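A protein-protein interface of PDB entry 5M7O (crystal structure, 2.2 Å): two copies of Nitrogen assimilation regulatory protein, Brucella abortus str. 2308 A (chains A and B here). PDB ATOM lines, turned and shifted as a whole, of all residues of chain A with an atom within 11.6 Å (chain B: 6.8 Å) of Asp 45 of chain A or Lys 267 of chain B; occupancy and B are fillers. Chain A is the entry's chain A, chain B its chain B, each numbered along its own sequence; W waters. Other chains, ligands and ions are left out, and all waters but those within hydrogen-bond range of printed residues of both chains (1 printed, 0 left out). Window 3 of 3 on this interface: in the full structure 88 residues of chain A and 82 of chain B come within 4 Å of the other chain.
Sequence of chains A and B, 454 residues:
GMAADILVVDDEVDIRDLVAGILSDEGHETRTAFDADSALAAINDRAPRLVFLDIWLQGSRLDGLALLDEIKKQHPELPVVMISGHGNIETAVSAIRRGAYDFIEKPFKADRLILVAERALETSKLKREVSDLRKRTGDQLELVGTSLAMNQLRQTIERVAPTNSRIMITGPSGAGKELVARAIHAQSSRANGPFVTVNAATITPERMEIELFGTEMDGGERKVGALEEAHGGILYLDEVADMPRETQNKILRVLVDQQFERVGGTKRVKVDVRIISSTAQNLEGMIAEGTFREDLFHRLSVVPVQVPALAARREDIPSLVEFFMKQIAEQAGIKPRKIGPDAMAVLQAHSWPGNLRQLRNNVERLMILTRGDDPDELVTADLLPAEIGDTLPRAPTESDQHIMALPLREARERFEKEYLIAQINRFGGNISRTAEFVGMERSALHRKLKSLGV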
ATOM      1  N   ASP A   5      34.129  31.069 -25.514  1.00  0.00           N
ATOM      2  CA  ASP A   5      32.790  31.517 -25.245  1.00  0.00           C
ATOM      3  C   ASP A   5      32.783  31.887 -23.744  1.00  0.00           C
ATOM      4  O   ASP A   5      32.820  30.966 -22.891  1.00  0.00           O
ATOM      5  CB  ASP A   5      31.813  30.390 -25.614  1.00  0.00           C
ATOM      6  CG  ASP A   5      30.384  30.629 -25.169  1.00  0.00           C
ATOM      7  OD1 ASP A   5      29.987  31.774 -24.834  1.00  0.00           O
ATOM      8  OD2 ASP A   5      29.643  29.613 -25.179  1.00  0.00           O
ATOM      9  N   LEU A   7      30.888  33.988 -20.714  1.00  0.00           N
ATOM     10  CA  LEU A   7      29.779  34.615 -20.015  1.00  0.00           C
ATOM     11  C   LEU A   7      30.276  35.687 -19.004  1.00  0.00           C
ATOM     12  O   LEU A   7      31.189  35.460 -18.193  1.00  0.00           O
ATOM     13  CB  LEU A   7      28.987  33.551 -19.277  1.00  0.00           C
ATOM     14  CG  LEU A   7      27.749  33.979 -18.541  1.00  0.00           C
ATOM     15  CD1 LEU A   7      26.745  34.510 -19.537  1.00  0.00           C
ATOM     16  CD2 LEU A   7      27.144  32.809 -17.767  1.00  0.00           C
ATOM     17  N   GLU A  29      33.917  35.185 -28.077  1.00  0.00           N
ATOM     18  CA  GLU A  29      32.474  35.276 -28.227  1.00  0.00           C
ATOM     19  C   GLU A  29      31.908  35.554 -26.839  1.00  0.00           C
ATOM     20  O   GLU A  29      32.080  34.745 -25.942  1.00  0.00           O
ATOM     21  CB  GLU A  29      31.902  33.945 -28.760  1.00  0.00           C
ATOM     22  CG  GLU A  29      30.355  33.869 -28.835  1.00  0.00           C
ATOM     23  CD  GLU A  29      29.773  32.440 -28.813  1.00  0.00           C
ATOM     24  OE1 GLU A  29      30.427  31.467 -29.271  1.00  0.00           O
ATOM     25  OE2 GLU A  29      28.635  32.291 -28.317  1.00  0.00           O
ATOM     26  N   THR A  30      31.188  36.656 -26.669  1.00  0.00           N
ATOM     27  CA  THR A  30      30.663  37.023 -25.356  1.00  0.00           C
ATOM     28  C   THR A  30      29.166  36.911 -25.202  1.00  0.00           C
ATOM     29  O   THR A  30      28.422  37.172 -26.114  1.00  0.00           O
ATOM     30  CB  THR A  30      31.045  38.452 -25.006  1.00  0.00           C
ATOM     31  OG1 THR A  30      30.645  39.302 -26.062  1.00  0.00           O
ATOM     32  CG2 THR A  30      32.550  38.572 -24.815  1.00  0.00           C
ATOM     33  N   ARG A  31      28.740  36.526 -24.012  1.00  0.00           N
ATOM     34  CA  ARG A  31      27.355  36.657 -23.593  1.00  0.00           C
ATOM     35  C   ARG A  31      27.312  37.304 -22.224  1.00  0.00           C
ATOM     36  O   ARG A  31      28.274  37.184 -21.435  1.00  0.00           O
ATOM     37  CB  ARG A  31      26.693  35.303 -23.519  1.00  0.00           C
ATOM     38  CG  ARG A  31      26.656  34.560 -24.852  1.00  0.00           C
ATOM     39  CD  ARG A  31      25.984  33.216 -24.630  1.00  0.00           C
ATOM     40  NE  ARG A  31      26.916  32.156 -24.234  1.00  0.00           N
ATOM     41  CZ  ARG A  31      26.579  31.077 -23.533  1.00  0.00           C
ATOM     42  NH1 ARG A  31      25.330  30.907 -23.079  1.00  0.00           N
ATOM     43  NH2 ARG A  31      27.507  30.158 -23.257  1.00  0.00           N
ATOM     44  N   THR A  32      26.204  37.985 -21.937  1.00  0.00           N
ATOM     45  CA  THR A  32      26.061  38.753 -20.707  1.00  0.00           C
ATOM     46  C   THR A  32      24.761  38.486 -19.966  1.00  0.00           C
ATOM     47  O   THR A  32      23.754  38.064 -20.525  1.00  0.00           O
ATOM     48  CB  THR A  32      26.200  40.272 -20.914  1.00  0.00           C
ATOM     49  OG1 THR A  32      24.982  40.821 -21.403  1.00  0.00           O
ATOM     50  CG2 THR A  32      27.333  40.627 -21.882  1.00  0.00           C
ATOM     51  N   ALA A  33      24.837  38.753 -18.677  1.00  0.00           N
ATOM     52  CA  ALA A  33      23.769  38.526 -17.734  1.00  0.00           C
ATOM     53  C   ALA A  33      24.010  39.459 -16.522  1.00  0.00           C
ATOM     54  O   ALA A  33      25.099  40.020 -16.349  1.00  0.00           O
ATOM     55  CB  ALA A  33      23.743  37.080 -17.285  1.00  0.00           C
ATOM     56  N   PHE A  34      22.980  39.598 -15.700  1.00  0.00           N
ATOM     57  CA  PHE A  34      22.975  40.593 -14.631  1.00  0.00           C
ATOM     58  C   PHE A  34      22.467  40.094 -13.288  1.00  0.00           C
ATOM     59  O   PHE A  34      22.506  40.837 -12.328  1.00  0.00           O
ATOM     60  CB  PHE A  34      22.160  41.800 -15.080  1.00  0.00           C
ATOM     61  CG  PHE A  34      20.745  41.463 -15.447  1.00  0.00           C
ATOM     62  CD1 PHE A  34      20.419  41.091 -16.763  1.00  0.00           C
ATOM     63  CD2 PHE A  34      19.734  41.489 -14.490  1.00  0.00           C
ATOM     64  CE1 PHE A  34      19.112  40.770 -17.113  1.00  0.00           C
ATOM     65  CE2 PHE A  34      18.416  41.172 -14.840  1.00  0.00           C
ATOM     66  CZ  PHE A  34      18.107  40.804 -16.147  1.00  0.00           C
ATOM     67  N   ALA A  36      21.175  36.063 -10.986  1.00  0.00           N
ATOM     68  CA  ALA A  36      21.259  34.609 -11.011  1.00  0.00           C
ATOM     69  C   ALA A  36      20.437  34.008 -12.156  1.00  0.00           C
ATOM     70  O   ALA A  36      20.969  33.248 -12.963  1.00  0.00           O
ATOM     71  CB  ALA A  36      20.816  34.021  -9.685  1.00  0.00           C
ATOM     72  N   ASP A  37      19.156  34.363 -12.238  1.00  0.00           N
ATOM     73  CA  ASP A  37      18.231  33.741 -13.204  1.00  0.00           C
ATOM     74  C   ASP A  37      18.719  33.893 -14.639  1.00  0.00           C
ATOM     75  O   ASP A  37      18.685  32.908 -15.395  1.00  0.00           O
ATOM     76  CB  ASP A  37      16.813  34.294 -13.075  1.00  0.00           C
ATOM     77  CG  ASP A  37      16.186  34.003 -11.704  1.00  0.00           C
ATOM     78  OD1 ASP A  37      16.543  32.983 -11.069  1.00  0.00           O
ATOM     79  OD2 ASP A  37      15.333  34.809 -11.257  1.00  0.00           O
ATOM     80  N   SER A  38      19.211  35.095 -14.987  1.00  0.00           N
ATOM     81  CA  SER A  38      19.779  35.319 -16.309  1.00  0.00           C
ATOM     82  C   SER A  38      21.100  34.568 -16.493  1.00  0.00           C
ATOM     83  O   SER A  38      21.349  34.026 -17.581  1.00  0.00           O
ATOM     84  CB  SER A  38      19.915  36.812 -16.666  1.00  0.00           C
ATOM     85  OG  SER A  38      20.688  37.546 -15.739  1.00  0.00           O
ATOM     86  N   ALA A  39      21.949  34.528 -15.463  1.00  0.00           N
ATOM     87  CA  ALA A  39      23.236  33.788 -15.553  1.00  0.00           C
ATOM     88  C   ALA A  39      23.024  32.283 -15.735  1.00  0.00           C
ATOM     89  O   ALA A  39      23.635  31.679 -16.629  1.00  0.00           O
ATOM     90  CB  ALA A  39      24.103  34.051 -14.339  1.00  0.00           C
ATOM     91  N   LEU A  40      22.126  31.699 -14.941  1.00  0.00           N
ATOM     92  CA  LEU A  40      21.796  30.257 -15.048  1.00  0.00           C
ATOM     93  C   LEU A  40      21.070  29.856 -16.346  1.00  0.00           C
ATOM     94  O   LEU A  40      21.235  28.746 -16.824  1.00  0.00           O
ATOM     95  CB  LEU A  40      20.968  29.798 -13.836  1.00  0.00           C
ATOM     96  CG  LEU A  40      21.641  29.979 -12.464  1.00  0.00           C
ATOM     97  CD1 LEU A  40      20.798  29.482 -11.297  1.00  0.00           C
ATOM     98  CD2 LEU A  40      22.980  29.281 -12.422  1.00  0.00           C
ATOM     99  N   ALA A  41      20.230  30.743 -16.875  1.00  0.00           N
ATOM    100  CA  ALA A  41      19.576  30.513 -18.159  1.00  0.00           C
ATOM    101  C   ALA A  41      20.612  30.526 -19.256  1.00  0.00           C
ATOM    102  O   ALA A  41      20.553  29.690 -20.155  1.00  0.00           O
ATOM    103  CB  ALA A  41      18.504  31.568 -18.432  1.00  0.00           C
ATOM    104  N   ALA A  42      21.572  31.455 -19.189  1.00  0.00           N
ATOM    105  CA  ALA A  42      22.643  31.483 -20.203  1.00  0.00           C
ATOM    106  C   ALA A  42      23.466  30.185 -20.163  1.00  0.00           C
ATOM    107  O   ALA A  42      23.823  29.653 -21.194  1.00  0.00           O
ATOM    108  CB  ALA A  42      23.544  32.696 -20.047  1.00  0.00           C
ATOM    109  N   ILE A  43      23.707  29.668 -18.964  1.00  0.00           N
ATOM    110  CA  ILE A  43      24.467  28.438 -18.789  1.00  0.00           C
ATOM    111  C   ILE A  43      23.667  27.226 -19.300  1.00  0.00           C
ATOM    112  O   ILE A  43      24.215  26.346 -19.960  1.00  0.00           O
ATOM    113  CB  ILE A  43      24.942  28.328 -17.321  1.00  0.00           C
ATOM    114  CG1 ILE A  43      26.134  29.281 -17.121  1.00  0.00           C
ATOM    115  CG2 ILE A  43      25.325  26.899 -16.936  1.00  0.00           C
ATOM    116  CD1 ILE A  43      26.367  29.656 -15.669  1.00  0.00           C
ATOM    117  N   ASN A  44      22.377  27.200 -19.014  1.00  0.00           N
ATOM    118  CA  ASN A  44      21.453  26.204 -19.595  1.00  0.00           C
ATOM    119  C   ASN A  44      21.327  26.281 -21.151  1.00  0.00           C
ATOM    120  O   ASN A  44      21.242  25.229 -21.810  1.00  0.00           O
ATOM    121  CB  ASN A  44      20.081  26.344 -18.939  1.00  0.00           C
ATOM    122  CG  ASN A  44      19.251  25.090 -19.035  1.00  0.00           C
ATOM    123  OD1 ASN A  44      19.694  24.003 -18.674  1.00  0.00           O
ATOM    124  ND2 ASN A  44      18.013  25.239 -19.496  1.00  0.00           N
ATOM    125  N   ASP A  45      21.348  27.489 -21.737  1.00  0.00           N
ATOM    126  CA  ASP A  45      21.261  27.629 -23.219  1.00  0.00           C
ATOM    127  C   ASP A  45      22.475  26.909 -23.783  1.00  0.00           C
ATOM    128  O   ASP A  45      22.390  26.189 -24.761  1.00  0.00           O
ATOM    129  CB  ASP A  45      21.327  29.093 -23.750  1.00  0.00           C
ATOM    130  CG  ASP A  45      20.143  30.030 -23.279  1.00  0.00           C
ATOM    131  OD1 ASP A  45      19.143  29.548 -22.692  1.00  0.00           O
ATOM    132  OD2 ASP A  45      20.232  31.285 -23.510  1.00  0.00           O
ATOM    133  N   ARG A  46      23.626  27.163 -23.176  1.00  0.00           N
ATOM    134  CA  ARG A  46      24.884  26.534 -23.559  1.00  0.00           C
ATOM    135  C   ARG A  46      25.922  26.744 -22.458  1.00  0.00           C
ATOM    136  O   ARG A  46      25.960  27.787 -21.849  1.00  0.00           O
ATOM    137  CB  ARG A  46      25.413  27.102 -24.888  1.00  0.00           C
ATOM    138  CG  ARG A  46      26.575  26.276 -25.418  1.00  0.00           C
ATOM    139  CD  ARG A  46      27.156  26.723 -26.746  1.00  0.00           C
ATOM    140  NE  ARG A  46      27.511  28.126 -26.737  1.00  0.00           N
ATOM    141  CZ  ARG A  46      26.835  29.088 -27.354  1.00  0.00           C
ATOM    142  NH1 ARG A  46      25.760  28.810 -28.076  1.00  0.00           N
ATOM    143  NH2 ARG A  46      27.239  30.343 -27.247  1.00  0.00           N
ATOM    144  N   ALA A  47      26.791  25.770 -22.238  1.00  0.00           N
ATOM    145  CA  ALA A  47      27.766  25.855 -21.172  1.00  0.00           C
ATOM    146  C   ALA A  47      28.885  26.698 -21.694  1.00  0.00           C
ATOM    147  O   ALA A  47      29.406  26.381 -22.734  1.00  0.00           O
ATOM    148  CB  ALA A  47      28.266  24.468 -20.820  1.00  0.00           C
ATOM    149  N   PRO A  48      29.260  27.783 -20.993  1.00  0.00           N
ATOM    150  CA  PRO A  48      30.367  28.568 -21.556  1.00  0.00           C
ATOM    151  C   PRO A  48      31.684  27.986 -21.164  1.00  0.00           C
ATOM    152  O   PRO A  48      31.740  27.097 -20.321  1.00  0.00           O
ATOM    153  CB  PRO A  48      30.210  29.932 -20.895  1.00  0.00           C
ATOM    154  CG  PRO A  48      29.632  29.601 -19.565  1.00  0.00           C
ATOM    155  CD  PRO A  48      28.732  28.401 -19.768  1.00  0.00           C
ATOM    156  N   ARG A  49      32.728  28.524 -21.757  1.00  0.00           N
ATOM    157  CA  ARG A  49      34.084  28.120 -21.463  1.00  0.00           C
ATOM    158  C   ARG A  49      34.673  28.807 -20.204  1.00  0.00           C
ATOM    159  O   ARG A  49      35.630  28.330 -19.600  1.00  0.00           O
ATOM    160  CB  ARG A  49      34.924  28.449 -22.709  1.00  0.00           C
ATOM    161  CG  ARG A  49      36.225  27.700 -22.872  1.00  0.00           C
ATOM    162  CD  ARG A  49      36.178  26.180 -22.647  1.00  0.00           C
ATOM    163  NE  ARG A  49      37.550  25.760 -22.367  1.00  0.00           N
ATOM    164  CZ  ARG A  49      38.158  25.786 -21.171  1.00  0.00           C
ATOM    165  NH1 ARG A  49      37.493  26.124 -20.049  1.00  0.00           N
ATOM    166  NH2 ARG A  49      39.438  25.392 -21.091  1.00  0.00           N
ATOM    167  N   GLN A  74      27.100  22.911 -10.701  1.00  0.00           N
ATOM    168  CA  GLN A  74      26.632  22.454 -12.002  1.00  0.00           C
ATOM    169  C   GLN A  74      27.764  22.056 -12.902  1.00  0.00           C
ATOM    170  O   GLN A  74      27.672  21.018 -13.554  1.00  0.00           O
ATOM    171  CB  GLN A  74      25.839  23.548 -12.690  1.00  0.00           C
ATOM    172  CG  GLN A  74      24.459  23.759 -12.094  1.00  0.00           C
ATOM    173  CD  GLN A  74      23.546  24.596 -12.994  1.00  0.00           C
ATOM    174  OE1 GLN A  74      23.621  24.526 -14.230  1.00  0.00           O
ATOM    175  NE2 GLN A  74      22.676  25.385 -12.379  1.00  0.00           N
ATOM    176  N   HIS A  75      28.783  22.921 -12.963  1.00  0.00           N
ATOM    177  CA  HIS A  75      29.991  22.732 -13.775  1.00  0.00           C
ATOM    178  C   HIS A  75      31.269  22.903 -12.959  1.00  0.00           C
ATOM    179  O   HIS A  75      31.886  23.971 -12.970  1.00  0.00           O
ATOM    180  CB  HIS A  75      30.016  23.684 -14.946  1.00  0.00           C
ATOM    181  CG  HIS A  75      28.903  23.450 -15.898  1.00  0.00           C
ATOM    182  ND1 HIS A  75      27.884  24.353 -16.086  1.00  0.00           N
ATOM    183  CD2 HIS A  75      28.614  22.386 -16.670  1.00  0.00           C
ATOM    184  CE1 HIS A  75      27.027  23.865 -16.962  1.00  0.00           C
ATOM    185  NE2 HIS A  75      27.444  22.668 -17.323  1.00  0.00           N
ATOM    186  N   LEU A  78      34.363  24.476 -14.724  1.00  0.00           N
ATOM    187  CA  LEU A  78      34.180  25.696 -15.508  1.00  0.00           C
ATOM    188  C   LEU A  78      34.900  26.823 -14.753  1.00  0.00           C
ATOM    189  O   LEU A  78      34.537  27.143 -13.645  1.00  0.00           O
ATOM    190  CB  LEU A  78      32.669  25.961 -15.696  1.00  0.00           C
ATOM    191  CG  LEU A  78      32.306  27.364 -16.173  1.00  0.00           C
ATOM    192  CD1 LEU A  78      33.016  27.710 -17.484  1.00  0.00           C
ATOM    193  CD2 LEU A  78      30.801  27.503 -16.283  1.00  0.00           C
ATOM    194  N   GLU B 228      28.406  19.955 -27.407  1.00  0.00           N
ATOM    195  CA  GLU B 228      28.481  21.177 -26.587  1.00  0.00           C
ATOM    196  C   GLU B 228      29.903  21.585 -26.269  1.00  0.00           C
ATOM    197  O   GLU B 228      30.252  22.734 -26.384  1.00  0.00           O
ATOM    198  CB  GLU B 228      27.705  20.983 -25.296  1.00  0.00           C
ATOM    199  CG  GLU B 228      27.354  22.276 -24.591  1.00  0.00           C
ATOM    200  CD  GLU B 228      26.260  22.100 -23.560  1.00  0.00           C
ATOM    201  OE1 GLU B 228      25.608  21.025 -23.520  1.00  0.00           O
ATOM    202  OE2 GLU B 228      26.016  23.058 -22.783  1.00  0.00           O
ATOM    203  N   PHE B 260      20.348  20.718 -30.585  1.00  0.00           N
ATOM    204  CA  PHE B 260      20.013  19.408 -30.086  1.00  0.00           C
ATOM    205  C   PHE B 260      19.495  19.471 -28.692  1.00  0.00           C
ATOM    206  O   PHE B 260      19.699  20.452 -28.003  1.00  0.00           O
ATOM    207  CB  PHE B 260      21.244  18.515 -30.151  1.00  0.00           C
ATOM    208  CG  PHE B 260      22.323  18.899 -29.206  1.00  0.00           C
ATOM    209  CD1 PHE B 260      22.346  18.378 -27.918  1.00  0.00           C
ATOM    210  CD2 PHE B 260      23.325  19.769 -29.591  1.00  0.00           C
ATOM    211  CE1 PHE B 260      23.332  18.741 -27.023  1.00  0.00           C
ATOM    212  CE2 PHE B 260      24.319  20.120 -28.699  1.00  0.00           C
ATOM    213  CZ  PHE B 260      24.320  19.609 -27.416  1.00  0.00           C
ATOM    214  N   GLU B 261      18.839  18.404 -28.269  1.00  0.00           N
ATOM    215  CA  GLU B 261      18.364  18.266 -26.894  1.00  0.00           C
ATOM    216  C   GLU B 261      19.384  17.415 -26.067  1.00  0.00           C
ATOM    217  O   GLU B 261      19.921  16.439 -26.538  1.00  0.00           O
ATOM    218  CB  GLU B 261      16.931  17.687 -26.885  1.00  0.00           C
ATOM    219  CG  GLU B 261      15.845  18.563 -27.578  1.00  0.00           C
ATOM    220  CD  GLU B 261      15.751  18.410 -29.123  1.00  0.00           C
ATOM    221  OE1 GLU B 261      15.754  17.262 -29.636  1.00  0.00           O
ATOM    222  OE2 GLU B 261      15.662  19.441 -29.851  1.00  0.00           O
ATOM    223  N   ARG B 262      19.693  17.843 -24.855  1.00  0.00           N
ATOM    224  CA  ARG B 262      20.483  17.036 -23.920  1.00  0.00           C
ATOM    225  C   ARG B 262      19.617  15.834 -23.513  1.00  0.00           C
ATOM    226  O   ARG B 262      18.388  15.937 -23.505  1.00  0.00           O
ATOM    227  CB  ARG B 262      20.853  17.856 -22.657  1.00  0.00           C
ATOM    228  CG  ARG B 262      21.582  19.185 -22.903  1.00  0.00           C
ATOM    229  CD  ARG B 262      22.425  19.685 -21.718  1.00  0.00           C
ATOM    230  NE  ARG B 262      23.126  20.933 -22.048  1.00  0.00           N
ATOM    231  CZ  ARG B 262      22.614  22.164 -21.914  1.00  0.00           C
ATOM    232  NH1 ARG B 262      21.379  22.360 -21.460  1.00  0.00           N
ATOM    233  NH2 ARG B 262      23.335  23.224 -22.253  1.00  0.00           N
ATOM    234  N   GLY B 265      16.803  16.422 -21.336  1.00  0.00           N
ATOM    235  CA  GLY B 265      16.621  17.881 -21.398  1.00  0.00           C
ATOM    236  C   GLY B 265      15.440  18.287 -22.288  1.00  0.00           C
ATOM    237  O   GLY B 265      14.941  17.494 -23.104  1.00  0.00           O
ATOM    238  N   THR B 266      14.973  19.518 -22.100  1.00  0.00           N
ATOM    239  CA  THR B 266      14.000  20.142 -23.012  1.00  0.00           C
ATOM    240  C   THR B 266      14.599  21.312 -23.786  1.00  0.00           C
ATOM    241  O   THR B 266      14.159  21.594 -24.889  1.00  0.00           O
ATOM    242  CB  THR B 266      12.755  20.658 -22.284  1.00  0.00           C
ATOM    243  OG1 THR B 266      13.101  21.854 -21.595  1.00  0.00           O
ATOM    244  CG2 THR B 266      12.195  19.617 -21.287  1.00  0.00           C
ATOM    245  N   LYS B 267      15.587  21.993 -23.221  1.00  0.00           N
ATOM    246  CA  LYS B 267      16.255  23.069 -23.926  1.00  0.00           C
ATOM    247  C   LYS B 267      16.916  22.583 -25.195  1.00  0.00           C
ATOM    248  O   LYS B 267      17.548  21.542 -25.206  1.00  0.00           O
ATOM    249  CB  LYS B 267      17.333  23.733 -23.055  1.00  0.00           C
ATOM    250  CG  LYS B 267      17.871  25.049 -23.639  1.00  0.00           C
ATOM    251  CD  LYS B 267      16.784  26.130 -23.641  1.00  0.00           C
ATOM    252  CE  LYS B 267      17.309  27.475 -24.081  1.00  0.00           C
ATOM    253  NZ  LYS B 267      17.972  27.471 -25.418  1.00  0.00           N
ATOM    254  N   ARG B 268      16.804  23.382 -26.242  1.00  0.00           N
ATOM    255  CA  ARG B 268      17.455  23.123 -27.514  1.00  0.00           C
ATOM    256  C   ARG B 268      18.722  23.923 -27.600  1.00  0.00           C
ATOM    257  O   ARG B 268      18.664  25.127 -27.745  1.00  0.00           O
ATOM    258  CB  ARG B 268      16.525  23.527 -28.664  1.00  0.00           C
ATOM    259  CG  ARG B 268      15.239  22.725 -28.723  1.00  0.00           C
ATOM    260  CD  ARG B 268      14.491  22.946 -30.029  1.00  0.00           C
ATOM    261  NE  ARG B 268      15.177  22.337 -31.167  1.00  0.00           N
ATOM    262  CZ  ARG B 268      15.050  22.711 -32.440  1.00  0.00           C
ATOM    263  NH1 ARG B 268      14.248  23.724 -32.804  1.00  0.00           N
ATOM    264  NH2 ARG B 268      15.747  22.055 -33.361  1.00  0.00           N
ATOM    265  N   VAL B 269      19.869  23.257 -27.560  1.00  0.00           N
ATOM    266  CA  VAL B 269      21.172  23.932 -27.447  1.00  0.00           C
ATOM    267  C   VAL B 269      21.771  24.259 -28.804  1.00  0.00           C
ATOM    268  O   VAL B 269      21.961  23.364 -29.605  1.00  0.00           O
ATOM    269  CB  VAL B 269      22.186  23.016 -26.691  1.00  0.00           C
ATOM    270  CG1 VAL B 269      23.549  23.698 -26.530  1.00  0.00           C
ATOM    271  CG2 VAL B 269      21.631  22.566 -25.343  1.00  0.00           C
ATOM    272  N   LYS B 270      22.140  25.511 -29.043  1.00  0.00           N
ATOM    273  CA  LYS B 270      22.773  25.898 -30.312  1.00  0.00           C
ATOM    274  C   LYS B 270      24.260  25.742 -30.239  1.00  0.00           C
ATOM    275  O   LYS B 270      24.866  26.182 -29.286  1.00  0.00           O
ATOM    276  CB  LYS B 270      22.463  27.340 -30.676  1.00  0.00           C
ATOM    277  CG  LYS B 270      20.980  27.609 -30.805  1.00  0.00           C
ATOM    278  CD  LYS B 270      20.649  28.935 -31.501  1.00  0.00           C
ATOM    279  CE  LYS B 270      19.405  29.643 -30.923  1.00  0.00           C
ATOM    280  NZ  LYS B 270      18.366  28.802 -30.232  1.00  0.00           N
HETATM  281  O   HOH W   1      25.847  21.929 -20.207  1.00  0.00           O
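The guanidinium group of Arg 262 of chain B sits at hydrogen-bond distance from the backbone carbonyl oxygen of Asn 44 of chain A (2.9 Å). The side-chain carboxylate (OD1) of Asp 45 of chain A lies within salt-bridge range of the side-chain amino group (NZ) of Lys 267 of chain B (3.6 Å). NH1 of Arg 46 of chain A sits at hydrogen-bond distance from O of Lys 270 of chain B, at 3.0 Å. OE2 of Glu 228 of chain B lies within hydrogen-bond range of N of Ala 47 of chain A (2.9 Å).
OD2 of Asp 5 of chain A is in salt-bridge range of NE of Arg 46 of chain A (3.0 Å). OE2 of Glu 29 of chain A is in salt-bridge range of NH2 of Arg 46 of chain A, 2.6 Å away. The backbone carbonyl oxygen of Arg 46 of chain A is in hydrogen-bond range of the guanidinium group of Arg 31 of chain A (3.2 Å). OE2 of Glu 228 of chain B is in salt-bridge range of NH2 of Arg 262 of chain B. The backbone carbonyl oxygen (O) of Phe 260 of chain B is in hydrogen-bond range of the backbone NH (N) of Val 269 of chain B (2.8 Å).
Among the printed residues, pairs that only touch across the chains: Ile 43 of chain A with Arg 262 of chain B (3.97 Å), Asn 44 of chain A with Lys 267 of chain B (3.8 Å), Asp 45 of chain A with Arg 262 of chain B (3.997 Å), Asp 45 of chain A with Val 269 of chain B (3.3 Å), Arg 46 of chain A with Glu 228 of chain B (3.7 Å) and Arg 46 of chain A with Arg 262 of chain B (3.9 Å).
Of the printed residues of chain B, Asp 45 of chain A touches Arg 262 (3.997 Å), Lys 267 (3.1 Å) and Val 269 (3.3 Å). Printed residues of chain B within 4 Å of Arg 46 of chain A: Glu 228, Arg 262 and Lys 270. Printed residues of chain A within 4 Å of Glu 228 of chain B: Arg 46 and Ala 47. No residue of chain A comes within 4 Å of Phe 260 of chain B. Glu 261 of chain B touches none of the printed residues of chain A. No residue of chain A comes within 4 Å of Gly 265 of chain B. No residue of chain A comes within 4 Å of Thr 266 of chain B. Of chain A, only Asn 44 (3.8 Å) and Asp 45 (3.1 Å) come within 4 Å of Lys 267 of chain B. Of chain A, only Asp 45 (3.3 Å) comes within 4 Å of Val 269 of chain B. Lys 270 of chain B touches just one residue of chain A: Arg 46. The nearest residue of chain A that does not touch Lys 267 of chain B is Ala 41 of chain A (5.6 Å).
Hydrophobic or aromatic side chains of chain A within 4 Å of the printed part of chain B: Ala 47. Of the 10 printed residues of chain B, 5 touch a printed residue of chain A. Hydrophobic or aromatic side chains of chain B within 4 Å of the printed part of chain A: Val 269. Among the printed residues, 10 pairs touch across the chains. Among the printed residues, Asp or Glu carboxylates within 4 Å of a Lys or Arg side-chain nitrogen of the other chain: Asp 45 of chain A with Lys 267 of chain B.
No position is printed for both chains. Of the 10 pairs that touch across the chains among the printed residues, none has its exchanged pair printed and touching as well.
Water W1 lies within hydrogen-bond range of OE2 of Glu 228 of chain B, NE2 of His 75 of chain A and NE of Arg 262 of chain B.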
